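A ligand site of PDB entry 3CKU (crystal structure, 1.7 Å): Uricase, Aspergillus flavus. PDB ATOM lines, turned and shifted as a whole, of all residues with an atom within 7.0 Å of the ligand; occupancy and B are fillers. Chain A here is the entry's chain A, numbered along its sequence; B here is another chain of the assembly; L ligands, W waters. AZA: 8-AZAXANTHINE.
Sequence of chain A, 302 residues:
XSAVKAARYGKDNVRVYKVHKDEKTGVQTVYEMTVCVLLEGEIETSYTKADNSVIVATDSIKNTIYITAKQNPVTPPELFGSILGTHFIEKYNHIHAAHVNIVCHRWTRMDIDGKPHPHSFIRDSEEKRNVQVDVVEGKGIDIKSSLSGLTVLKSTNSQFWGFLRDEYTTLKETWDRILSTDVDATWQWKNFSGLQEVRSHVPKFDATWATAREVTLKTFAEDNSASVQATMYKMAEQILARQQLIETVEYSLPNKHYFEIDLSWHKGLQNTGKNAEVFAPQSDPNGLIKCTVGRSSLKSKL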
ATOM      1  N   SER A 158     -18.020  17.662  -8.503  1.00  0.00           N
ATOM      2  CA  SER A 158     -19.367  17.872  -8.020  1.00  0.00           C
ATOM      3  C   SER A 158     -19.319  19.141  -7.149  1.00  0.00           C
ATOM      4  O   SER A 158     -18.358  19.221  -6.394  1.00  0.00           O
ATOM      5  CB  SER A 158     -19.918  16.695  -7.242  1.00  0.00           C
ATOM      6  OG  SER A 158     -21.104  17.027  -6.548  1.00  0.00           O
ATOM      7  N   GLN A 159     -20.266  20.045  -7.290  1.00  0.00           N
ATOM      8  CA  GLN A 159     -20.298  21.284  -6.542  1.00  0.00           C
ATOM      9  C   GLN A 159     -21.689  21.532  -5.978  1.00  0.00           C
ATOM     10  O   GLN A 159     -22.652  20.987  -6.507  1.00  0.00           O
ATOM     11  CB  GLN A 159     -19.913  22.452  -7.482  1.00  0.00           C
ATOM     12  CG  GLN A 159     -18.540  22.237  -8.108  1.00  0.00           C
ATOM     13  CD  GLN A 159     -18.143  23.373  -9.039  1.00  0.00           C
ATOM     14  OE1 GLN A 159     -18.314  24.542  -8.696  1.00  0.00           O
ATOM     15  NE2 GLN A 159     -17.603  23.013 -10.202  1.00  0.00           N
ATOM     16  N   PHE A 160     -21.779  22.376  -4.932  1.00  0.00           N
ATOM     17  CA  PHE A 160     -23.096  22.797  -4.484  1.00  0.00           C
ATOM     18  C   PHE A 160     -22.939  24.158  -3.805  1.00  0.00           C
ATOM     19  O   PHE A 160     -22.514  24.243  -2.651  1.00  0.00           O
ATOM     20  CB  PHE A 160     -23.793  21.759  -3.600  1.00  0.00           C
ATOM     21  CG  PHE A 160     -25.283  22.127  -3.432  1.00  0.00           C
ATOM     22  CD1 PHE A 160     -26.077  22.220  -4.572  1.00  0.00           C
ATOM     23  CD2 PHE A 160     -25.837  22.370  -2.194  1.00  0.00           C
ATOM     24  CE1 PHE A 160     -27.413  22.551  -4.414  1.00  0.00           C
ATOM     25  CE2 PHE A 160     -27.170  22.715  -2.047  1.00  0.00           C
ATOM     26  CZ  PHE A 160     -27.966  22.822  -3.187  1.00  0.00           C
ATOM     27  N   PHE A 163     -27.082  28.175  -3.178  1.00  0.00           N
ATOM     28  CA  PHE A 163     -28.421  27.880  -2.685  1.00  0.00           C
ATOM     29  C   PHE A 163     -28.944  28.930  -1.708  1.00  0.00           C
ATOM     30  O   PHE A 163     -28.205  29.791  -1.216  1.00  0.00           O
ATOM     31  CB  PHE A 163     -28.451  26.510  -1.984  1.00  0.00           C
ATOM     32  CG  PHE A 163     -27.255  26.239  -1.085  1.00  0.00           C
ATOM     33  CD1 PHE A 163     -26.054  25.779  -1.557  1.00  0.00           C
ATOM     34  CD2 PHE A 163     -27.427  26.469   0.276  1.00  0.00           C
ATOM     35  CE1 PHE A 163     -25.002  25.523  -0.665  1.00  0.00           C
ATOM     36  CE2 PHE A 163     -26.415  26.212   1.163  1.00  0.00           C
ATOM     37  CZ  PHE A 163     -25.219  25.748   0.674  1.00  0.00           C
ATOM     38  N   LEU A 171     -25.410  24.735   6.102  1.00  0.00           N
ATOM     39  CA  LEU A 171     -24.549  24.096   5.123  1.00  0.00           C
ATOM     40  C   LEU A 171     -23.571  25.058   4.473  1.00  0.00           C
ATOM     41  O   LEU A 171     -23.975  26.104   3.941  1.00  0.00           O
ATOM     42  CB  LEU A 171     -25.420  23.455   4.025  1.00  0.00           C
ATOM     43  CG  LEU A 171     -24.707  22.712   2.896  1.00  0.00           C
ATOM     44  CD1 LEU A 171     -23.998  21.463   3.377  1.00  0.00           C
ATOM     45  CD2 LEU A 171     -25.734  22.363   1.824  1.00  0.00           C
ATOM     46  N   ARG A 177     -16.851  18.463  -4.036  1.00  0.00           N
ATOM     47  CA  ARG A 177     -17.356  17.525  -3.046  1.00  0.00           C
ATOM     48  C   ARG A 177     -17.482  16.154  -3.739  1.00  0.00           C
ATOM     49  O   ARG A 177     -17.329  16.100  -4.948  1.00  0.00           O
ATOM     50  CB  ARG A 177     -18.722  17.915  -2.485  1.00  0.00           C
ATOM     51  CG  ARG A 177     -19.767  18.059  -3.586  1.00  0.00           C
ATOM     52  CD  ARG A 177     -21.152  18.337  -3.017  1.00  0.00           C
ATOM     53  NE  ARG A 177     -22.188  18.121  -4.055  1.00  0.00           N
ATOM     54  CZ  ARG A 177     -23.483  18.204  -3.859  1.00  0.00           C
ATOM     55  NH1 ARG A 177     -24.035  18.505  -2.681  1.00  0.00           N
ATOM     56  NH2 ARG A 177     -24.311  17.978  -4.893  1.00  0.00           N
ATOM     57  N   LEU A 179     -19.847  13.070  -4.886  1.00  0.00           N
ATOM     58  CA  LEU A 179     -21.255  12.801  -5.192  1.00  0.00           C
ATOM     59  C   LEU A 179     -21.409  11.295  -5.410  1.00  0.00           C
ATOM     60  O   LEU A 179     -20.708  10.710  -6.232  1.00  0.00           O
ATOM     61  CB  LEU A 179     -21.697  13.550  -6.431  1.00  0.00           C
ATOM     62  CG  LEU A 179     -23.152  13.327  -6.884  1.00  0.00           C
ATOM     63  CD1 LEU A 179     -24.132  13.654  -5.774  1.00  0.00           C
ATOM     64  CD2 LEU A 179     -23.439  14.131  -8.156  1.00  0.00           C
ATOM     65  N   SER A 225     -20.758  18.763 -11.935  1.00  0.00           N
ATOM     66  CA  SER A 225     -22.121  18.931 -11.476  1.00  0.00           C
ATOM     67  C   SER A 225     -22.385  20.147 -10.615  1.00  0.00           C
ATOM     68  O   SER A 225     -21.761  20.365  -9.572  1.00  0.00           O
ATOM     69  CB  SER A 225     -22.472  17.633 -10.701  1.00  0.00           C
ATOM     70  OG  SER A 225     -23.729  17.854 -10.088  1.00  0.00           O
ATOM     71  N   ALA A 226     -23.353  20.964 -11.022  1.00  0.00           N
ATOM     72  CA  ALA A 226     -23.797  22.111 -10.210  1.00  0.00           C
ATOM     73  C   ALA A 226     -24.699  21.719  -9.055  1.00  0.00           C
ATOM     74  O   ALA A 226     -24.894  22.474  -8.101  1.00  0.00           O
ATOM     75  CB  ALA A 226     -24.554  23.096 -11.105  1.00  0.00           C
ATOM     76  N   SER A 227     -25.295  20.517  -9.185  1.00  0.00           N
ATOM     77  CA  SER A 227     -26.206  19.917  -8.241  1.00  0.00           C
ATOM     78  C   SER A 227     -26.768  18.603  -8.797  1.00  0.00           C
ATOM     79  O   SER A 227     -26.594  18.311  -9.970  1.00  0.00           O
ATOM     80  CB  SER A 227     -27.406  20.807  -7.872  1.00  0.00           C
ATOM     81  OG  SER A 227     -28.224  21.002  -9.028  1.00  0.00           O
ATOM     82  N   VAL A 228     -27.424  17.840  -7.915  1.00  0.00           N
ATOM     83  CA  VAL A 228     -28.024  16.598  -8.423  1.00  0.00           C
ATOM     84  C   VAL A 228     -29.104  16.950  -9.434  1.00  0.00           C
ATOM     85  O   VAL A 228     -29.225  16.347 -10.496  1.00  0.00           O
ATOM     86  CB  VAL A 228     -28.570  15.792  -7.236  1.00  0.00           C
ATOM     87  CG1 VAL A 228     -29.290  14.527  -7.684  1.00  0.00           C
ATOM     88  CG2 VAL A 228     -27.421  15.365  -6.299  1.00  0.00           C
ATOM     89  N   GLN A 229     -29.882  17.969  -9.084  1.00  0.00           N
ATOM     90  CA  GLN A 229     -30.970  18.440  -9.937  1.00  0.00           C
ATOM     91  C   GLN A 229     -30.521  18.668 -11.370  1.00  0.00           C
ATOM     92  O   GLN A 229     -31.069  18.208 -12.373  1.00  0.00           O
ATOM     93  CB  GLN A 229     -31.485  19.759  -9.324  1.00  0.00           C
ATOM     94  CG  GLN A 229     -32.332  19.691  -8.098  1.00  0.00           C
ATOM     95  CD  GLN A 229     -31.643  19.668  -6.761  1.00  0.00           C
ATOM     96  OE1 GLN A 229     -30.472  19.286  -6.668  1.00  0.00           O
ATOM     97  NE2 GLN A 229     -32.371  20.063  -5.725  1.00  0.00           N
ATOM     98  N   ALA A 230     -29.425  19.437 -11.524  1.00  0.00           N
ATOM     99  CA  ALA A 230     -28.969  19.863 -12.835  1.00  0.00           C
ATOM    100  C   ALA A 230     -28.393  18.706 -13.637  1.00  0.00           C
ATOM    101  O   ALA A 230     -28.553  18.656 -14.855  1.00  0.00           O
ATOM    102  CB  ALA A 230     -27.953  20.994 -12.693  1.00  0.00           C
ATOM    103  N   ASN A 255     -28.977  11.516  -2.478  1.00  0.00           N
ATOM    104  CA  ASN A 255     -27.620  12.069  -2.379  1.00  0.00           C
ATOM    105  C   ASN A 255     -27.035  11.429  -1.119  1.00  0.00           C
ATOM    106  O   ASN A 255     -27.437  11.806  -0.026  1.00  0.00           O
ATOM    107  CB  ASN A 255     -27.682  13.577  -2.285  1.00  0.00           C
ATOM    108  CG  ASN A 255     -26.352  14.289  -2.441  1.00  0.00           C
ATOM    109  OD1 ASN A 255     -25.304  13.683  -2.618  1.00  0.00           O
ATOM    110  ND2 ASN A 255     -26.372  15.614  -2.418  1.00  0.00           N
ATOM    111  N   HIS A 257     -24.536  11.197   1.327  1.00  0.00           N
ATOM    112  CA  HIS A 257     -23.515  12.154   1.694  1.00  0.00           C
ATOM    113  C   HIS A 257     -22.237  11.516   2.249  1.00  0.00           C
ATOM    114  O   HIS A 257     -22.316  10.550   3.008  1.00  0.00           O
ATOM    115  CB  HIS A 257     -24.061  13.138   2.752  1.00  0.00           C
ATOM    116  CG  HIS A 257     -25.383  13.776   2.377  1.00  0.00           C
ATOM    117  ND1 HIS A 257     -25.520  14.609   1.292  1.00  0.00           N
ATOM    118  CD2 HIS A 257     -26.600  13.701   2.940  1.00  0.00           C
ATOM    119  CE1 HIS A 257     -26.802  15.016   1.217  1.00  0.00           C
ATOM    120  NE2 HIS A 257     -27.496  14.478   2.211  1.00  0.00           N
ATOM    121  N   GLY A 287     -30.209  13.262   1.114  1.00  0.00           N
ATOM    122  CA  GLY A 287     -31.107  13.971   0.196  1.00  0.00           C
ATOM    123  C   GLY A 287     -31.831  13.010  -0.724  1.00  0.00           C
ATOM    124  O   GLY A 287     -31.341  11.924  -1.052  1.00  0.00           O
ATOM    125  N   ILE A 289     -33.770  13.465  -4.457  1.00  0.00           N
ATOM    126  CA  ILE A 289     -34.045  14.433  -5.530  1.00  0.00           C
ATOM    127  C   ILE A 289     -34.785  13.754  -6.668  1.00  0.00           C
ATOM    128  O   ILE A 289     -34.340  12.733  -7.166  1.00  0.00           O
ATOM    129  CB  ILE A 289     -32.735  15.035  -6.076  1.00  0.00           C
ATOM    130  CG1 ILE A 289     -31.714  15.448  -5.008  1.00  0.00           C
ATOM    131  CG2 ILE A 289     -32.993  16.213  -7.008  1.00  0.00           C
ATOM    132  CD1 ILE A 289     -32.260  16.368  -3.939  1.00  0.00           C
ATOM    133  N   TYR B   9     -38.076  17.463  -4.151  1.00  0.00           N
ATOM    134  CA  TYR B   9     -36.716  17.170  -3.679  1.00  0.00           C
ATOM    135  C   TYR B   9     -36.735  17.424  -2.179  1.00  0.00           C
ATOM    136  O   TYR B   9     -37.546  18.240  -1.720  1.00  0.00           O
ATOM    137  CB  TYR B   9     -35.652  18.028  -4.416  1.00  0.00           C
ATOM    138  CG  TYR B   9     -35.546  19.376  -3.701  1.00  0.00           C
ATOM    139  CD1 TYR B   9     -36.555  20.304  -3.913  1.00  0.00           C
ATOM    140  CD2 TYR B   9     -34.484  19.689  -2.854  1.00  0.00           C
ATOM    141  CE1 TYR B   9     -36.508  21.542  -3.294  1.00  0.00           C
ATOM    142  CE2 TYR B   9     -34.456  20.927  -2.211  1.00  0.00           C
ATOM    143  CZ  TYR B   9     -35.462  21.838  -2.445  1.00  0.00           C
ATOM    144  OH  TYR B   9     -35.417  23.056  -1.803  1.00  0.00           O
ATOM    145  N   GLY B  10     -35.829  16.806  -1.415  1.00  0.00           N
ATOM    146  CA  GLY B  10     -35.696  17.158   0.001  1.00  0.00           C
ATOM    147  C   GLY B  10     -34.824  16.139   0.745  1.00  0.00           C
ATOM    148  O   GLY B  10     -33.901  15.609   0.138  1.00  0.00           O
ATOM    149  N   LYS B  11     -35.142  15.945   2.014  1.00  0.00           N
ATOM    150  CA  LYS B  11     -34.310  15.036   2.829  1.00  0.00           C
ATOM    151  C   LYS B  11     -35.162  13.859   3.296  1.00  0.00           C
ATOM    152  O   LYS B  11     -36.232  14.093   3.849  1.00  0.00           O
ATOM    153  CB  LYS B  11     -33.706  15.775   4.017  1.00  0.00           C
ATOM    154  CG  LYS B  11     -32.613  14.954   4.730  1.00  0.00           C
ATOM    155  CD  LYS B  11     -31.309  14.962   3.956  1.00  0.00           C
ATOM    156  CE  LYS B  11     -30.327  16.026   4.433  1.00  0.00           C
ATOM    157  NZ  LYS B  11     -29.286  16.292   3.393  1.00  0.00           N
ATOM    158  N   ASN B  52     -29.315  27.463  -8.400  1.00  0.00           N
ATOM    159  CA  ASN B  52     -29.597  26.951  -7.060  1.00  0.00           C
ATOM    160  C   ASN B  52     -30.243  27.945  -6.114  1.00  0.00           C
ATOM    161  O   ASN B  52     -30.572  27.603  -4.968  1.00  0.00           O
ATOM    162  CB  ASN B  52     -28.292  26.413  -6.433  1.00  0.00           C
ATOM    163  CG  ASN B  52     -27.794  25.160  -7.133  1.00  0.00           C
ATOM    164  OD1 ASN B  52     -28.573  24.392  -7.690  1.00  0.00           O
ATOM    165  ND2 ASN B  52     -26.478  24.954  -7.129  1.00  0.00           N
ATOM    166  N   ILE B  55     -33.308  26.749  -4.504  1.00  0.00           N
ATOM    167  CA  ILE B  55     -33.218  25.592  -3.622  1.00  0.00           C
ATOM    168  C   ILE B  55     -33.028  25.954  -2.151  1.00  0.00           C
ATOM    169  O   ILE B  55     -32.023  26.603  -1.851  1.00  0.00           O
ATOM    170  CB  ILE B  55     -32.026  24.687  -4.035  1.00  0.00           C
ATOM    171  CG1 ILE B  55     -32.168  24.193  -5.472  1.00  0.00           C
ATOM    172  CG2 ILE B  55     -31.891  23.534  -3.069  1.00  0.00           C
ATOM    173  CD1 ILE B  55     -31.055  23.275  -5.932  1.00  0.00           C
ATOM    174  N   VAL B  56     -33.975  25.524  -1.356  1.00  0.00           N
ATOM    175  CA  VAL B  56     -33.872  25.448   0.104  1.00  0.00           C
ATOM    176  C   VAL B  56     -33.005  24.195   0.303  1.00  0.00           C
ATOM    177  O   VAL B  56     -33.512  23.122  -0.032  1.00  0.00           O
ATOM    178  CB  VAL B  56     -35.212  25.326   0.824  1.00  0.00           C
ATOM    179  CG1 VAL B  56     -35.038  25.152   2.324  1.00  0.00           C
ATOM    180  CG2 VAL B  56     -36.085  26.557   0.570  1.00  0.00           C
ATOM    181  N   ALA B  57     -31.766  24.284   0.768  1.00  0.00           N
ATOM    182  CA  ALA B  57     -30.933  23.068   0.792  1.00  0.00           C
ATOM    183  C   ALA B  57     -31.571  21.945   1.606  1.00  0.00           C
ATOM    184  O   ALA B  57     -32.224  22.171   2.620  1.00  0.00           O
ATOM    185  CB  ALA B  57     -29.569  23.386   1.391  1.00  0.00           C
ATOM    186  N   THR B  58     -31.389  20.697   1.145  1.00  0.00           N
ATOM    187  CA  THR B  58     -32.001  19.594   1.903  1.00  0.00           C
ATOM    188  C   THR B  58     -31.382  19.500   3.299  1.00  0.00           C
ATOM    189  O   THR B  58     -32.018  19.060   4.239  1.00  0.00           O
ATOM    190  CB  THR B  58     -31.836  18.240   1.191  1.00  0.00           C
ATOM    191  OG1 THR B  58     -30.452  17.861   1.217  1.00  0.00           O
ATOM    192  CG2 THR B  58     -32.221  18.377  -0.279  1.00  0.00           C
ATOM    193  N   ASP B  59     -30.125  19.961   3.396  1.00  0.00           N
ATOM    194  CA  ASP B  59     -29.548  20.062   4.739  1.00  0.00           C
ATOM    195  C   ASP B  59     -30.332  21.007   5.619  1.00  0.00           C
ATOM    196  O   ASP B  59     -30.498  20.767   6.813  1.00  0.00           O
ATOM    197  CB  ASP B  59     -28.091  20.536   4.636  1.00  0.00           C
ATOM    198  CG  ASP B  59     -27.395  20.443   5.990  1.00  0.00           C
ATOM    199  OD1 ASP B  59     -26.952  19.328   6.374  1.00  0.00           O
ATOM    200  OD2 ASP B  59     -27.297  21.467   6.669  1.00  0.00           O
ATOM    201  N   SER B  60     -30.815  22.135   5.043  1.00  0.00           N
ATOM    202  CA  SER B  60     -31.634  23.060   5.809  1.00  0.00           C
ATOM    203  C   SER B  60     -33.010  22.483   6.132  1.00  0.00           C
ATOM    204  O   SER B  60     -33.589  22.783   7.165  1.00  0.00           O
ATOM    205  CB  SER B  60     -31.823  24.387   5.043  1.00  0.00           C
ATOM    206  OG  SER B  60     -30.539  24.864   4.638  1.00  0.00           O
HETATM  207  N1  AZA L   1     -28.921  19.357  -4.125  1.00  0.00           N
HETATM  208  C2  AZA L   1     -27.619  18.914  -4.136  1.00  0.00           C
HETATM  209  O2  AZA L   1     -27.114  18.515  -5.152  1.00  0.00           O
HETATM  210  N3  AZA L   1     -26.935  18.960  -2.939  1.00  0.00           N
HETATM  211  C4  AZA L   1     -27.600  19.396  -1.842  1.00  0.00           C
HETATM  212  C5  AZA L   1     -28.898  19.880  -1.853  1.00  0.00           C
HETATM  213  C6  AZA L   1     -29.665  19.838  -3.074  1.00  0.00           C
HETATM  214  O6  AZA L   1     -30.823  20.221  -3.245  1.00  0.00           O
HETATM  215  N7  AZA L   1     -29.274  20.303  -0.666  1.00  0.00           N
HETATM  216  N8  AZA L   1     -28.230  20.097   0.109  1.00  0.00           N
HETATM  217  N9  AZA L   1     -27.149  19.546  -0.555  1.00  0.00           N
HETATM  218  O   HOH W   1     -24.791  18.471   0.560  1.00  0.00           O
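Water W1 bridges N9 of the ligand and NH1 of Arg 177.
The side-chain amino group (NZ) of Lys 11 of chain B is in hydrogen-bond range of the side-chain hydroxyl (OG1) of Thr 58 of chain B (2.9 Å). The backbone NH (N) of Arg 177 is in hydrogen-bond range of the backbone carbonyl oxygen (O) of Ser 158, 2.9 Å away. The backbone NH of Gln 229 sits close to the side-chain hydroxyl of Ser 227, at 3.5 Å. The backbone carbonyl oxygen (O) of Asn 255 lies within hydrogen-bond range of a ring nitrogen (NE2) of His 257 (3.5 Å). N of Asn 255 sits at hydrogen-bond distance from O of Gly 287, at 2.8 Å. O of Ser 227 lies within hydrogen-bond range of OG of Ser 225 (2.9 Å). The backbone NH (N) of Ala 230 lies within hydrogen-bond range of the side-chain hydroxyl (OG) of Ser 227 (3.2 Å). The backbone carbonyl oxygen of Val 56 of chain B sits at hydrogen-bond distance from the side-chain hydroxyl of Tyr 9 of chain B (2.6 Å).
The backbone NH of Thr 58 of chain B is in hydrogen-bond range of a nitrogen (N7) of the ligand (2.8 Å). The side-chain hydroxyl (OG1) of Thr 58 of chain B sits at hydrogen-bond distance from a nitrogen (N7) of the ligand, at 3.3 Å. The backbone NH (N) of Val 228 sits at hydrogen-bond distance from an oxygen (O2) of the ligand (2.9 Å). The guanidinium group (NH2) of Arg 177 is in hydrogen-bond range of an oxygen (O2) of the ligand. The side-chain amide nitrogen (NE2) of Gln 229 is in hydrogen-bond range of an oxygen (O6) of the ligand, 2.9 Å away. ND2 of Asn 255 lies close to N3 of the ligand (3.4 Å).
Merely in contact with the ligand: Phe 160, Ile 55 of chain B, Ser 227, Ala 57 of chain B, Tyr 9 of chain B, Leu 171 and Asp 59 of chain B. The nearest printed residue that does not touch the ligand is Ile 289 (4.2 Å).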
